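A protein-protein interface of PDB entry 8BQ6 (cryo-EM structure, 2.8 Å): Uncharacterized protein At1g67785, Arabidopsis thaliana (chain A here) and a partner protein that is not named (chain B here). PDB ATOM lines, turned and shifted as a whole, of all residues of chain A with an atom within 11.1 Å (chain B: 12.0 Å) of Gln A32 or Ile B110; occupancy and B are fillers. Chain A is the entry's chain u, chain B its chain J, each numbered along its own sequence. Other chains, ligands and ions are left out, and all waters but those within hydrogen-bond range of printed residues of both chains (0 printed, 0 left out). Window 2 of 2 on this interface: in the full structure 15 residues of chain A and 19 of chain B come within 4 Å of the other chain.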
ATOM      1  N   VAL A  24     -28.575 -11.413  20.968  1.00  0.00           N
ATOM      2  CA  VAL A  24     -27.642 -10.403  20.464  1.00  0.00           C
ATOM      3  C   VAL A  24     -26.651 -11.020  19.482  1.00  0.00           C
ATOM      4  O   VAL A  24     -26.298 -10.414  18.460  1.00  0.00           O
ATOM      5  CB  VAL A  24     -26.909  -9.710  21.630  1.00  0.00           C
ATOM      6  CG1 VAL A  24     -26.012  -8.609  21.103  1.00  0.00           C
ATOM      7  CG2 VAL A  24     -27.898  -9.135  22.619  1.00  0.00           C
ATOM      8  N   HIS A  25     -26.158 -12.220  19.790  1.00  0.00           N
ATOM      9  CA  HIS A  25     -25.197 -12.864  18.901  1.00  0.00           C
ATOM     10  C   HIS A  25     -25.830 -13.208  17.562  1.00  0.00           C
ATOM     11  O   HIS A  25     -25.194 -13.070  16.509  1.00  0.00           O
ATOM     12  CB  HIS A  25     -24.619 -14.110  19.561  1.00  0.00           C
ATOM     13  CG  HIS A  25     -23.759 -13.806  20.743  1.00  0.00           C
ATOM     14  ND1 HIS A  25     -22.784 -12.833  20.717  1.00  0.00           N
ATOM     15  CD2 HIS A  25     -23.736 -14.329  21.991  1.00  0.00           C
ATOM     16  CE1 HIS A  25     -22.194 -12.773  21.896  1.00  0.00           C
ATOM     17  NE2 HIS A  25     -22.753 -13.671  22.687  1.00  0.00           N
ATOM     18  N   VAL A  26     -27.084 -13.653  17.581  1.00  0.00           N
ATOM     19  CA  VAL A  26     -27.763 -13.953  16.324  1.00  0.00           C
ATOM     20  C   VAL A  26     -27.990 -12.676  15.522  1.00  0.00           C
ATOM     21  O   VAL A  26     -27.849 -12.663  14.291  1.00  0.00           O
ATOM     22  CB  VAL A  26     -29.075 -14.707  16.599  1.00  0.00           C
ATOM     23  CG1 VAL A  26     -29.869 -14.881  15.321  1.00  0.00           C
ATOM     24  CG2 VAL A  26     -28.761 -16.051  17.214  1.00  0.00           C
ATOM     25  N   TRP A  27     -28.326 -11.579  16.203  1.00  0.00           N
ATOM     26  CA  TRP A  27     -28.484 -10.303  15.512  1.00  0.00           C
ATOM     27  C   TRP A  27     -27.184  -9.870  14.843  1.00  0.00           C
ATOM     28  O   TRP A  27     -27.187  -9.419  13.692  1.00  0.00           O
ATOM     29  CB  TRP A  27     -28.960  -9.234  16.489  1.00  0.00           C
ATOM     30  CG  TRP A  27     -29.190  -7.911  15.847  1.00  0.00           C
ATOM     31  CD1 TRP A  27     -30.338  -7.468  15.257  1.00  0.00           C
ATOM     32  CD2 TRP A  27     -28.243  -6.850  15.728  1.00  0.00           C
ATOM     33  NE1 TRP A  27     -30.161  -6.196  14.775  1.00  0.00           N
ATOM     34  CE2 TRP A  27     -28.881  -5.794  15.051  1.00  0.00           C
ATOM     35  CE3 TRP A  27     -26.912  -6.692  16.124  1.00  0.00           C
ATOM     36  CZ2 TRP A  27     -28.235  -4.600  14.762  1.00  0.00           C
ATOM     37  CZ3 TRP A  27     -26.275  -5.504  15.840  1.00  0.00           C
ATOM     38  CH2 TRP A  27     -26.936  -4.472  15.168  1.00  0.00           C
ATOM     39  N   ILE A  28     -26.059  -9.989  15.554  1.00  0.00           N
ATOM     40  CA  ILE A  28     -24.779  -9.613  14.954  1.00  0.00           C
ATOM     41  C   ILE A  28     -24.458 -10.514  13.767  1.00  0.00           C
ATOM     42  O   ILE A  28     -23.971 -10.045  12.729  1.00  0.00           O
ATOM     43  CB  ILE A  28     -23.645  -9.635  15.997  1.00  0.00           C
ATOM     44  CG1 ILE A  28     -23.875  -8.563  17.061  1.00  0.00           C
ATOM     45  CG2 ILE A  28     -22.303  -9.408  15.313  1.00  0.00           C
ATOM     46  CD1 ILE A  28     -22.603  -8.030  17.691  1.00  0.00           C
ATOM     47  N   ALA A  29     -24.719 -11.816  13.897  1.00  0.00           N
ATOM     48  CA  ALA A  29     -24.454 -12.733  12.791  1.00  0.00           C
ATOM     49  C   ALA A  29     -25.315 -12.409  11.576  1.00  0.00           C
ATOM     50  O   ALA A  29     -24.889 -12.613  10.433  1.00  0.00           O
ATOM     51  CB  ALA A  29     -24.685 -14.175  13.237  1.00  0.00           C
ATOM     52  N   LEU A  30     -26.532 -11.911  11.801  1.00  0.00           N
ATOM     53  CA  LEU A  30     -27.434 -11.639  10.689  1.00  0.00           C
ATOM     54  C   LEU A  30     -27.038 -10.402   9.897  1.00  0.00           C
ATOM     55  O   LEU A  30     -27.487 -10.245   8.758  1.00  0.00           O
ATOM     56  CB  LEU A  30     -28.869 -11.492  11.191  1.00  0.00           C
ATOM     57  CG  LEU A  30     -29.628 -12.815  11.275  1.00  0.00           C
ATOM     58  CD1 LEU A  30     -30.802 -12.732  12.241  1.00  0.00           C
ATOM     59  CD2 LEU A  30     -30.088 -13.237   9.892  1.00  0.00           C
ATOM     60  N   HIS A  31     -26.212  -9.524  10.463  1.00  0.00           N
ATOM     61  CA  HIS A  31     -25.838  -8.282   9.802  1.00  0.00           C
ATOM     62  C   HIS A  31     -24.386  -8.267   9.349  1.00  0.00           C
ATOM     63  O   HIS A  31     -23.754  -7.206   9.357  1.00  0.00           O
ATOM     64  CB  HIS A  31     -26.109  -7.088  10.716  1.00  0.00           C
ATOM     65  CG  HIS A  31     -27.544  -6.952  11.114  1.00  0.00           C
ATOM     66  ND1 HIS A  31     -28.532  -6.599  10.222  1.00  0.00           N
ATOM     67  CD2 HIS A  31     -28.156  -7.108  12.311  1.00  0.00           C
ATOM     68  CE1 HIS A  31     -29.693  -6.554  10.848  1.00  0.00           C
ATOM     69  NE2 HIS A  31     -29.491  -6.851  12.118  1.00  0.00           N
ATOM     70  N   GLN A  32     -23.840  -9.417   8.958  1.00  0.00           N
ATOM     71  CA  GLN A  32     -22.489  -9.425   8.414  1.00  0.00           C
ATOM     72  C   GLN A  32     -22.469  -8.862   6.997  1.00  0.00           C
ATOM     73  O   GLN A  32     -21.471  -8.272   6.565  1.00  0.00           O
ATOM     74  CB  GLN A  32     -21.917 -10.841   8.448  1.00  0.00           C
ATOM     75  CG  GLN A  32     -21.353 -11.230   9.804  1.00  0.00           C
ATOM     76  CD  GLN A  32     -20.395 -10.188  10.353  1.00  0.00           C
ATOM     77  OE1 GLN A  32     -20.724  -9.453  11.284  1.00  0.00           O
ATOM     78  NE2 GLN A  32     -19.200 -10.124   9.779  1.00  0.00           N
ATOM     79  N   ASP A  33     -23.577  -9.014   6.268  1.00  0.00           N
ATOM     80  CA  ASP A  33     -23.605  -8.610   4.867  1.00  0.00           C
ATOM     81  C   ASP A  33     -23.666  -7.097   4.718  1.00  0.00           C
ATOM     82  O   ASP A  33     -23.017  -6.535   3.829  1.00  0.00           O
ATOM     83  CB  ASP A  33     -24.783  -9.271   4.160  1.00  0.00           C
ATOM     84  CG  ASP A  33     -24.616 -10.765   4.054  1.00  0.00           C
ATOM     85  OD1 ASP A  33     -24.404 -11.254   2.926  1.00  0.00           O
ATOM     86  OD2 ASP A  33     -24.683 -11.448   5.099  1.00  0.00           O
ATOM     87  N   GLU A  34     -24.447  -6.418   5.558  1.00  0.00           N
ATOM     88  CA  GLU A  34     -24.450  -4.960   5.520  1.00  0.00           C
ATOM     89  C   GLU A  34     -23.094  -4.402   5.924  1.00  0.00           C
ATOM     90  O   GLU A  34     -22.630  -3.411   5.351  1.00  0.00           O
ATOM     91  CB  GLU A  34     -25.555  -4.408   6.417  1.00  0.00           C
ATOM     92  CG  GLU A  34     -26.941  -4.582   5.832  1.00  0.00           C
ATOM     93  CD  GLU A  34     -27.562  -5.910   6.213  1.00  0.00           C
ATOM     94  OE1 GLU A  34     -26.906  -6.951   6.000  1.00  0.00           O
ATOM     95  OE2 GLU A  34     -28.700  -5.916   6.723  1.00  0.00           O
ATOM     96  N   LYS A  35     -22.443  -5.020   6.912  1.00  0.00           N
ATOM     97  CA  LYS A  35     -21.086  -4.607   7.250  1.00  0.00           C
ATOM     98  C   LYS A  35     -20.164  -4.752   6.050  1.00  0.00           C
ATOM     99  O   LYS A  35     -19.379  -3.846   5.742  1.00  0.00           O
ATOM    100  CB  LYS A  35     -20.555  -5.433   8.419  1.00  0.00           C
ATOM    101  CG  LYS A  35     -20.896  -4.885   9.783  1.00  0.00           C
ATOM    102  CD  LYS A  35     -20.403  -5.827  10.869  1.00  0.00           C
ATOM    103  CE  LYS A  35     -18.972  -6.278  10.611  1.00  0.00           C
ATOM    104  NZ  LYS A  35     -17.984  -5.195  10.867  1.00  0.00           N
ATOM    105  N   GLN A  36     -20.264  -5.881   5.348  1.00  0.00           N
ATOM    106  CA  GLN A  36     -19.403  -6.113   4.197  1.00  0.00           C
ATOM    107  C   GLN A  36     -19.684  -5.108   3.084  1.00  0.00           C
ATOM    108  O   GLN A  36     -18.753  -4.584   2.465  1.00  0.00           O
ATOM    109  CB  GLN A  36     -19.584  -7.553   3.715  1.00  0.00           C
ATOM    110  CG  GLN A  36     -18.727  -7.955   2.534  1.00  0.00           C
ATOM    111  CD  GLN A  36     -19.546  -8.306   1.312  1.00  0.00           C
ATOM    112  OE1 GLN A  36     -20.778  -8.286   1.345  1.00  0.00           O
ATOM    113  NE2 GLN A  36     -18.865  -8.648   0.226  1.00  0.00           N
ATOM    114  N   GLU A  37     -20.961  -4.804   2.836  1.00  0.00           N
ATOM    115  CA  GLU A  37     -21.307  -3.875   1.763  1.00  0.00           C
ATOM    116  C   GLU A  37     -20.886  -2.447   2.102  1.00  0.00           C
ATOM    117  O   GLU A  37     -20.411  -1.713   1.229  1.00  0.00           O
ATOM    118  CB  GLU A  37     -22.806  -3.958   1.449  1.00  0.00           C
ATOM    119  CG  GLU A  37     -23.284  -5.270   0.838  1.00  0.00           C
ATOM    120  CD  GLU A  37     -24.785  -5.317   0.617  1.00  0.00           C
ATOM    121  OE1 GLU A  37     -25.491  -4.411   1.109  1.00  0.00           O
ATOM    122  OE2 GLU A  37     -25.258  -6.266  -0.045  1.00  0.00           O
ATOM    123  N   ARG A  38     -21.039  -2.037   3.365  1.00  0.00           N
ATOM    124  CA  ARG A  38     -20.573  -0.716   3.773  1.00  0.00           C
ATOM    125  C   ARG A  38     -19.060  -0.615   3.662  1.00  0.00           C
ATOM    126  O   ARG A  38     -18.527   0.406   3.206  1.00  0.00           O
ATOM    127  CB  ARG A  38     -21.020  -0.417   5.203  1.00  0.00           C
ATOM    128  CG  ARG A  38     -21.141   1.060   5.521  1.00  0.00           C
ATOM    129  CD  ARG A  38     -22.437   1.625   4.975  1.00  0.00           C
ATOM    130  NE  ARG A  38     -22.822   2.863   5.639  1.00  0.00           N
ATOM    131  CZ  ARG A  38     -22.595   4.075   5.151  1.00  0.00           C
ATOM    132  NH1 ARG A  38     -21.962   4.251   4.003  1.00  0.00           N
ATOM    133  NH2 ARG A  38     -23.017   5.137   5.831  1.00  0.00           N
ATOM    134  N   MET A  39     -18.350  -1.670   4.068  1.00  0.00           N
ATOM    135  CA  MET A  39     -16.898  -1.682   3.946  1.00  0.00           C
ATOM    136  C   MET A  39     -16.468  -1.612   2.486  1.00  0.00           C
ATOM    137  O   MET A  39     -15.512  -0.906   2.149  1.00  0.00           O
ATOM    138  CB  MET A  39     -16.335  -2.933   4.617  1.00  0.00           C
ATOM    139  CG  MET A  39     -15.318  -2.661   5.714  1.00  0.00           C
ATOM    140  SD  MET A  39     -15.792  -1.306   6.806  1.00  0.00           S
ATOM    141  CE  MET A  39     -17.283  -1.974   7.542  1.00  0.00           C
ATOM    142  N   GLU A  40     -17.221  -2.264   1.595  1.00  0.00           N
ATOM    143  CA  GLU A  40     -16.918  -2.161   0.141  1.00  0.00           C
ATOM    144  C   GLU A  40     -16.845  -0.679  -0.230  1.00  0.00           C
ATOM    145  O   GLU A  40     -15.809  -0.263  -0.786  1.00  0.00           O
ATOM    146  CB  GLU A  40     -17.995  -2.860  -0.689  1.00  0.00           C
ATOM    147  CG  GLU A  40     -17.931  -4.379  -0.668  1.00  0.00           C
ATOM    148  CD  GLU A  40     -16.554  -5.012  -0.566  1.00  0.00           C
ATOM    149  OE1 GLU A  40     -15.852  -5.063  -1.595  1.00  0.00           O
ATOM    150  OE2 GLU A  40     -16.194  -5.474   0.538  1.00  0.00           O
ATOM    151  N   TRP B  99     -19.095  -4.240  25.520  1.00  0.00           N
ATOM    152  CA  TRP B  99     -19.276  -3.941  24.104  1.00  0.00           C
ATOM    153  C   TRP B  99     -18.021  -4.232  23.297  1.00  0.00           C
ATOM    154  O   TRP B  99     -18.115  -4.574  22.113  1.00  0.00           O
ATOM    155  CB  TRP B  99     -19.685  -2.479  23.923  1.00  0.00           C
ATOM    156  CG  TRP B  99     -19.638  -2.014  22.499  1.00  0.00           C
ATOM    157  CD1 TRP B  99     -18.870  -1.009  21.990  1.00  0.00           C
ATOM    158  CD2 TRP B  99     -20.393  -2.540  21.398  1.00  0.00           C
ATOM    159  NE1 TRP B  99     -19.098  -0.875  20.642  1.00  0.00           N
ATOM    160  CE2 TRP B  99     -20.028  -1.803  20.254  1.00  0.00           C
ATOM    161  CE3 TRP B  99     -21.338  -3.562  21.270  1.00  0.00           C
ATOM    162  CZ2 TRP B  99     -20.578  -2.055  18.997  1.00  0.00           C
ATOM    163  CZ3 TRP B  99     -21.883  -3.812  20.020  1.00  0.00           C
ATOM    164  CH2 TRP B  99     -21.501  -3.061  18.902  1.00  0.00           C
ATOM    165  N   PHE B 102     -16.941  -8.816  24.709  1.00  0.00           N
ATOM    166  CA  PHE B 102     -17.883  -9.909  24.519  1.00  0.00           C
ATOM    167  C   PHE B 102     -18.148 -10.164  23.045  1.00  0.00           C
ATOM    168  O   PHE B 102     -18.742 -11.190  22.699  1.00  0.00           O
ATOM    169  CB  PHE B 102     -19.208  -9.619  25.228  1.00  0.00           C
ATOM    170  CG  PHE B 102     -19.140  -9.751  26.716  1.00  0.00           C
ATOM    171  CD1 PHE B 102     -18.197  -9.053  27.445  1.00  0.00           C
ATOM    172  CD2 PHE B 102     -20.014 -10.583  27.389  1.00  0.00           C
ATOM    173  CE1 PHE B 102     -18.134  -9.169  28.808  1.00  0.00           C
ATOM    174  CE2 PHE B 102     -19.949 -10.706  28.755  1.00  0.00           C
ATOM    175  CZ  PHE B 102     -19.008  -9.998  29.464  1.00  0.00           C
ATOM    176  N   PHE B 103     -17.707  -9.256  22.176  1.00  0.00           N
ATOM    177  CA  PHE B 103     -17.961  -9.329  20.744  1.00  0.00           C
ATOM    178  C   PHE B 103     -16.687  -9.207  19.923  1.00  0.00           C
ATOM    179  O   PHE B 103     -16.738  -8.729  18.784  1.00  0.00           O
ATOM    180  CB  PHE B 103     -18.954  -8.240  20.341  1.00  0.00           C
ATOM    181  CG  PHE B 103     -20.060  -8.051  21.328  1.00  0.00           C
ATOM    182  CD1 PHE B 103     -20.119  -6.919  22.117  1.00  0.00           C
ATOM    183  CD2 PHE B 103     -21.044  -9.013  21.468  1.00  0.00           C
ATOM    184  CE1 PHE B 103     -21.139  -6.754  23.031  1.00  0.00           C
ATOM    185  CE2 PHE B 103     -22.066  -8.850  22.375  1.00  0.00           C
ATOM    186  CZ  PHE B 103     -22.115  -7.722  23.158  1.00  0.00           C
ATOM    187  N   ILE B 104     -15.560  -9.636  20.511  1.00  0.00           N
ATOM    188  CA  ILE B 104     -14.232  -9.521  19.828  1.00  0.00           C
ATOM    189  C   ILE B 104     -14.113 -10.633  18.781  1.00  0.00           C
ATOM    190  O   ILE B 104     -13.528 -10.376  17.714  1.00  0.00           O
ATOM    191  CB  ILE B 104     -13.090  -9.557  20.875  1.00  0.00           C
ATOM    192  CG1 ILE B 104     -11.725  -9.194  20.292  1.00  0.00           C
ATOM    193  CG2 ILE B 104     -13.028 -10.888  21.598  1.00  0.00           C
ATOM    194  CD1 ILE B 104     -10.853  -8.425  21.246  1.00  0.00           C
ATOM    195  N   LEU B 105     -14.669 -11.809  19.068  1.00  0.00           N
ATOM    196  CA  LEU B 105     -14.615 -12.928  18.138  1.00  0.00           C
ATOM    197  C   LEU B 105     -15.628 -12.802  17.005  1.00  0.00           C
ATOM    198  O   LEU B 105     -15.459 -13.467  15.978  1.00  0.00           O
ATOM    199  CB  LEU B 105     -14.837 -14.249  18.892  1.00  0.00           C
ATOM    200  CG  LEU B 105     -13.939 -14.603  20.090  1.00  0.00           C
ATOM    201  CD1 LEU B 105     -14.077 -16.069  20.474  1.00  0.00           C
ATOM    202  CD2 LEU B 105     -12.482 -14.285  19.811  1.00  0.00           C
ATOM    203  N   ASP B 106     -16.643 -11.940  17.147  1.00  0.00           N
ATOM    204  CA  ASP B 106     -17.783 -11.968  16.231  1.00  0.00           C
ATOM    205  C   ASP B 106     -17.361 -11.678  14.794  1.00  0.00           C
ATOM    206  O   ASP B 106     -17.837 -12.329  13.858  1.00  0.00           O
ATOM    207  CB  ASP B 106     -18.855 -10.974  16.686  1.00  0.00           C
ATOM    208  CG  ASP B 106     -19.566 -11.418  17.958  1.00  0.00           C
ATOM    209  OD1 ASP B 106     -18.920 -12.049  18.818  1.00  0.00           O
ATOM    210  OD2 ASP B 106     -20.777 -11.152  18.093  1.00  0.00           O
ATOM    211  N   ASN B 107     -16.473 -10.701  14.598  1.00  0.00           N
ATOM    212  CA  ASN B 107     -15.932 -10.435  13.272  1.00  0.00           C
ATOM    213  C   ASN B 107     -15.020 -11.554  12.794  1.00  0.00           C
ATOM    214  O   ASN B 107     -15.013 -11.881  11.602  1.00  0.00           O
ATOM    215  CB  ASN B 107     -15.156  -9.118  13.270  1.00  0.00           C
ATOM    216  CG  ASN B 107     -16.056  -7.911  13.390  1.00  0.00           C
ATOM    217  OD1 ASN B 107     -17.238  -7.975  13.062  1.00  0.00           O
ATOM    218  ND2 ASN B 107     -15.500  -6.798  13.853  1.00  0.00           N
ATOM    219  N   GLU B 108     -14.237 -12.138  13.697  1.00  0.00           N
ATOM    220  CA  GLU B 108     -13.285 -13.155  13.278  1.00  0.00           C
ATOM    221  C   GLU B 108     -13.915 -14.540  13.254  1.00  0.00           C
ATOM    222  O   GLU B 108     -13.678 -15.314  12.321  1.00  0.00           O
ATOM    223  CB  GLU B 108     -12.063 -13.133  14.194  1.00  0.00           C
ATOM    224  CG  GLU B 108     -10.908 -13.950  13.671  1.00  0.00           C
ATOM    225  CD  GLU B 108     -10.186 -13.242  12.551  1.00  0.00           C
ATOM    226  OE1 GLU B 108     -10.656 -13.330  11.397  1.00  0.00           O
ATOM    227  OE2 GLU B 108      -9.158 -12.589  12.823  1.00  0.00           O
ATOM    228  N   SER B 109     -14.724 -14.866  14.255  1.00  0.00           N
ATOM    229  CA  SER B 109     -15.369 -16.172  14.358  1.00  0.00           C
ATOM    230  C   SER B 109     -16.877 -15.956  14.263  1.00  0.00           C
ATOM    231  O   SER B 109     -17.568 -15.810  15.273  1.00  0.00           O
ATOM    232  CB  SER B 109     -14.983 -16.869  15.650  1.00  0.00           C
ATOM    233  OG  SER B 109     -15.456 -16.142  16.768  1.00  0.00           O
ATOM    234  N   ILE B 110     -17.378 -15.943  13.038  1.00  0.00           N
ATOM    235  CA  ILE B 110     -18.799 -15.689  12.802  1.00  0.00           C
ATOM    236  C   ILE B 110     -19.591 -16.939  13.173  1.00  0.00           C
ATOM    237  O   ILE B 110     -19.260 -18.034  12.697  1.00  0.00           O
ATOM    238  CB  ILE B 110     -19.033 -15.302  11.350  1.00  0.00           C
ATOM    239  CG1 ILE B 110     -18.407 -13.938  11.076  1.00  0.00           C
ATOM    240  CG2 ILE B 110     -20.513 -15.268  11.041  1.00  0.00           C
ATOM    241  CD1 ILE B 110     -18.175 -13.675   9.624  1.00  0.00           C
ATOM    242  N   PRO B 111     -20.611 -16.824  14.015  1.00  0.00           N
ATOM    243  CA  PRO B 111     -21.381 -18.008  14.399  1.00  0.00           C
ATOM    244  C   PRO B 111     -22.197 -18.570  13.249  1.00  0.00           C
ATOM    245  O   PRO B 111     -22.725 -17.841  12.406  1.00  0.00           O
ATOM    246  CB  PRO B 111     -22.290 -17.489  15.518  1.00  0.00           C
ATOM    247  CG  PRO B 111     -22.412 -16.046  15.258  1.00  0.00           C
ATOM    248  CD  PRO B 111     -21.113 -15.602  14.661  1.00  0.00           C
ATOM    249  N   LEU B 112     -22.308 -19.892  13.241  1.00  0.00           N
ATOM    250  CA  LEU B 112     -23.148 -20.608  12.291  1.00  0.00           C
ATOM    251  C   LEU B 112     -24.569 -20.661  12.841  1.00  0.00           C
ATOM    252  O   LEU B 112     -24.815 -21.280  13.880  1.00  0.00           O
ATOM    253  CB  LEU B 112     -22.602 -22.011  12.057  1.00  0.00           C
ATOM    254  CG  LEU B 112     -23.325 -22.809  10.988  1.00  0.00           C
ATOM    255  CD1 LEU B 112     -23.073 -22.170   9.642  1.00  0.00           C
ATOM    256  CD2 LEU B 112     -22.832 -24.237  11.018  1.00  0.00           C
ATOM    257  N   LEU B 113     -25.497 -20.016  12.146  1.00  0.00           N
ATOM    258  CA  LEU B 113     -26.880 -19.977  12.606  1.00  0.00           C
ATOM    259  C   LEU B 113     -27.543 -21.335  12.399  1.00  0.00           C
ATOM    260  O   LEU B 113     -27.361 -21.956  11.346  1.00  0.00           O
ATOM    261  CB  LEU B 113     -27.655 -18.898  11.860  1.00  0.00           C
ATOM    262  CG  LEU B 113     -27.198 -17.455  12.067  1.00  0.00           C
ATOM    263  CD1 LEU B 113     -27.819 -16.577  11.008  1.00  0.00           C
ATOM    264  CD2 LEU B 113     -27.554 -16.954  13.457  1.00  0.00           C
ATOM    265  N   PRO B 114     -28.320 -21.823  13.367  1.00  0.00           N
ATOM    266  CA  PRO B 114     -28.978 -23.132  13.219  1.00  0.00           C
ATOM    267  C   PRO B 114     -30.196 -23.033  12.312  1.00  0.00           C
ATOM    268  O   PRO B 114     -31.127 -22.269  12.577  1.00  0.00           O
ATOM    269  CB  PRO B 114     -29.372 -23.494  14.654  1.00  0.00           C
ATOM    270  CG  PRO B 114     -29.528 -22.187  15.339  1.00  0.00           C
ATOM    271  CD  PRO B 114     -28.604 -21.201  14.671  1.00  0.00           C
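His A25 touches Phe B102. His A25 touches Phe B103. His A25 touches Asp B106 (ND1 to OD2, 3.7 Å). Leu B113 touches Val A26 (CD2 to CG1, 3.6 Å). Ile A28 touches Asp B106. CB of Ala A29 touches CG of Pro B111 (3.6 Å). CD1 of Ile B110 touches NE2 of Gln A32 (3.7 Å). OD1 of Asn B107 touches CE of Lys A35 (3.4 Å).
Printed residues of chain B within 4 Å of His A25: Phe B102, Phe B103 and Asp B106. Of chain B, only Asp B106 comes within 4 Å of Ile A28. Printed residues of chain B within 4 Å of Ala A29: Pro B111 (3.6 Å). Gln A32 touches one residue of chain B. No residue of chain B comes within 4 Å of Glu A34. Of chain B, only Asn B107 (3.4 Å) comes within 4 Å of Lys A35. No residue of chain B comes within 4 Å of Gln A36. Printed residues of chain A within 4 Å of Phe B102: His A25 (3.9 Å). Of the printed residues of chain A, Phe B103 touches His A25. Asp B106 touches two residues of chain A. No residue of chain A comes within 4 Å of Ser B109. Of the printed residues of chain A, Ile B110 touches Gln A32 (3.7 Å). Of the printed residues of chain A, Leu B113 touches Val A26. The nearest residue of chain A that does not touch Ile B110 is Ala A29 (4.8 Å). The nearest printed residue of chain B that does not touch His A25 is Pro B111 (4.3 Å).
Printed residues of chain A that touch a printed residue of chain B: His A25, Val A26, Ile A28, Ala A29, Gln A32 and Lys A35. Hydrophobic or aromatic side chains of chain A within 4 Å of the printed part of chain B: His A25, Val A26, Ile A28 and Ala A29. Hydrophobic or aromatic side chains of chain B that line the printed part of chain A: Phe B103, Ile B110, Pro B111 and Leu B113. Along chain B the printed residues that touch a printed residue of chain A span positions 102 to 113.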
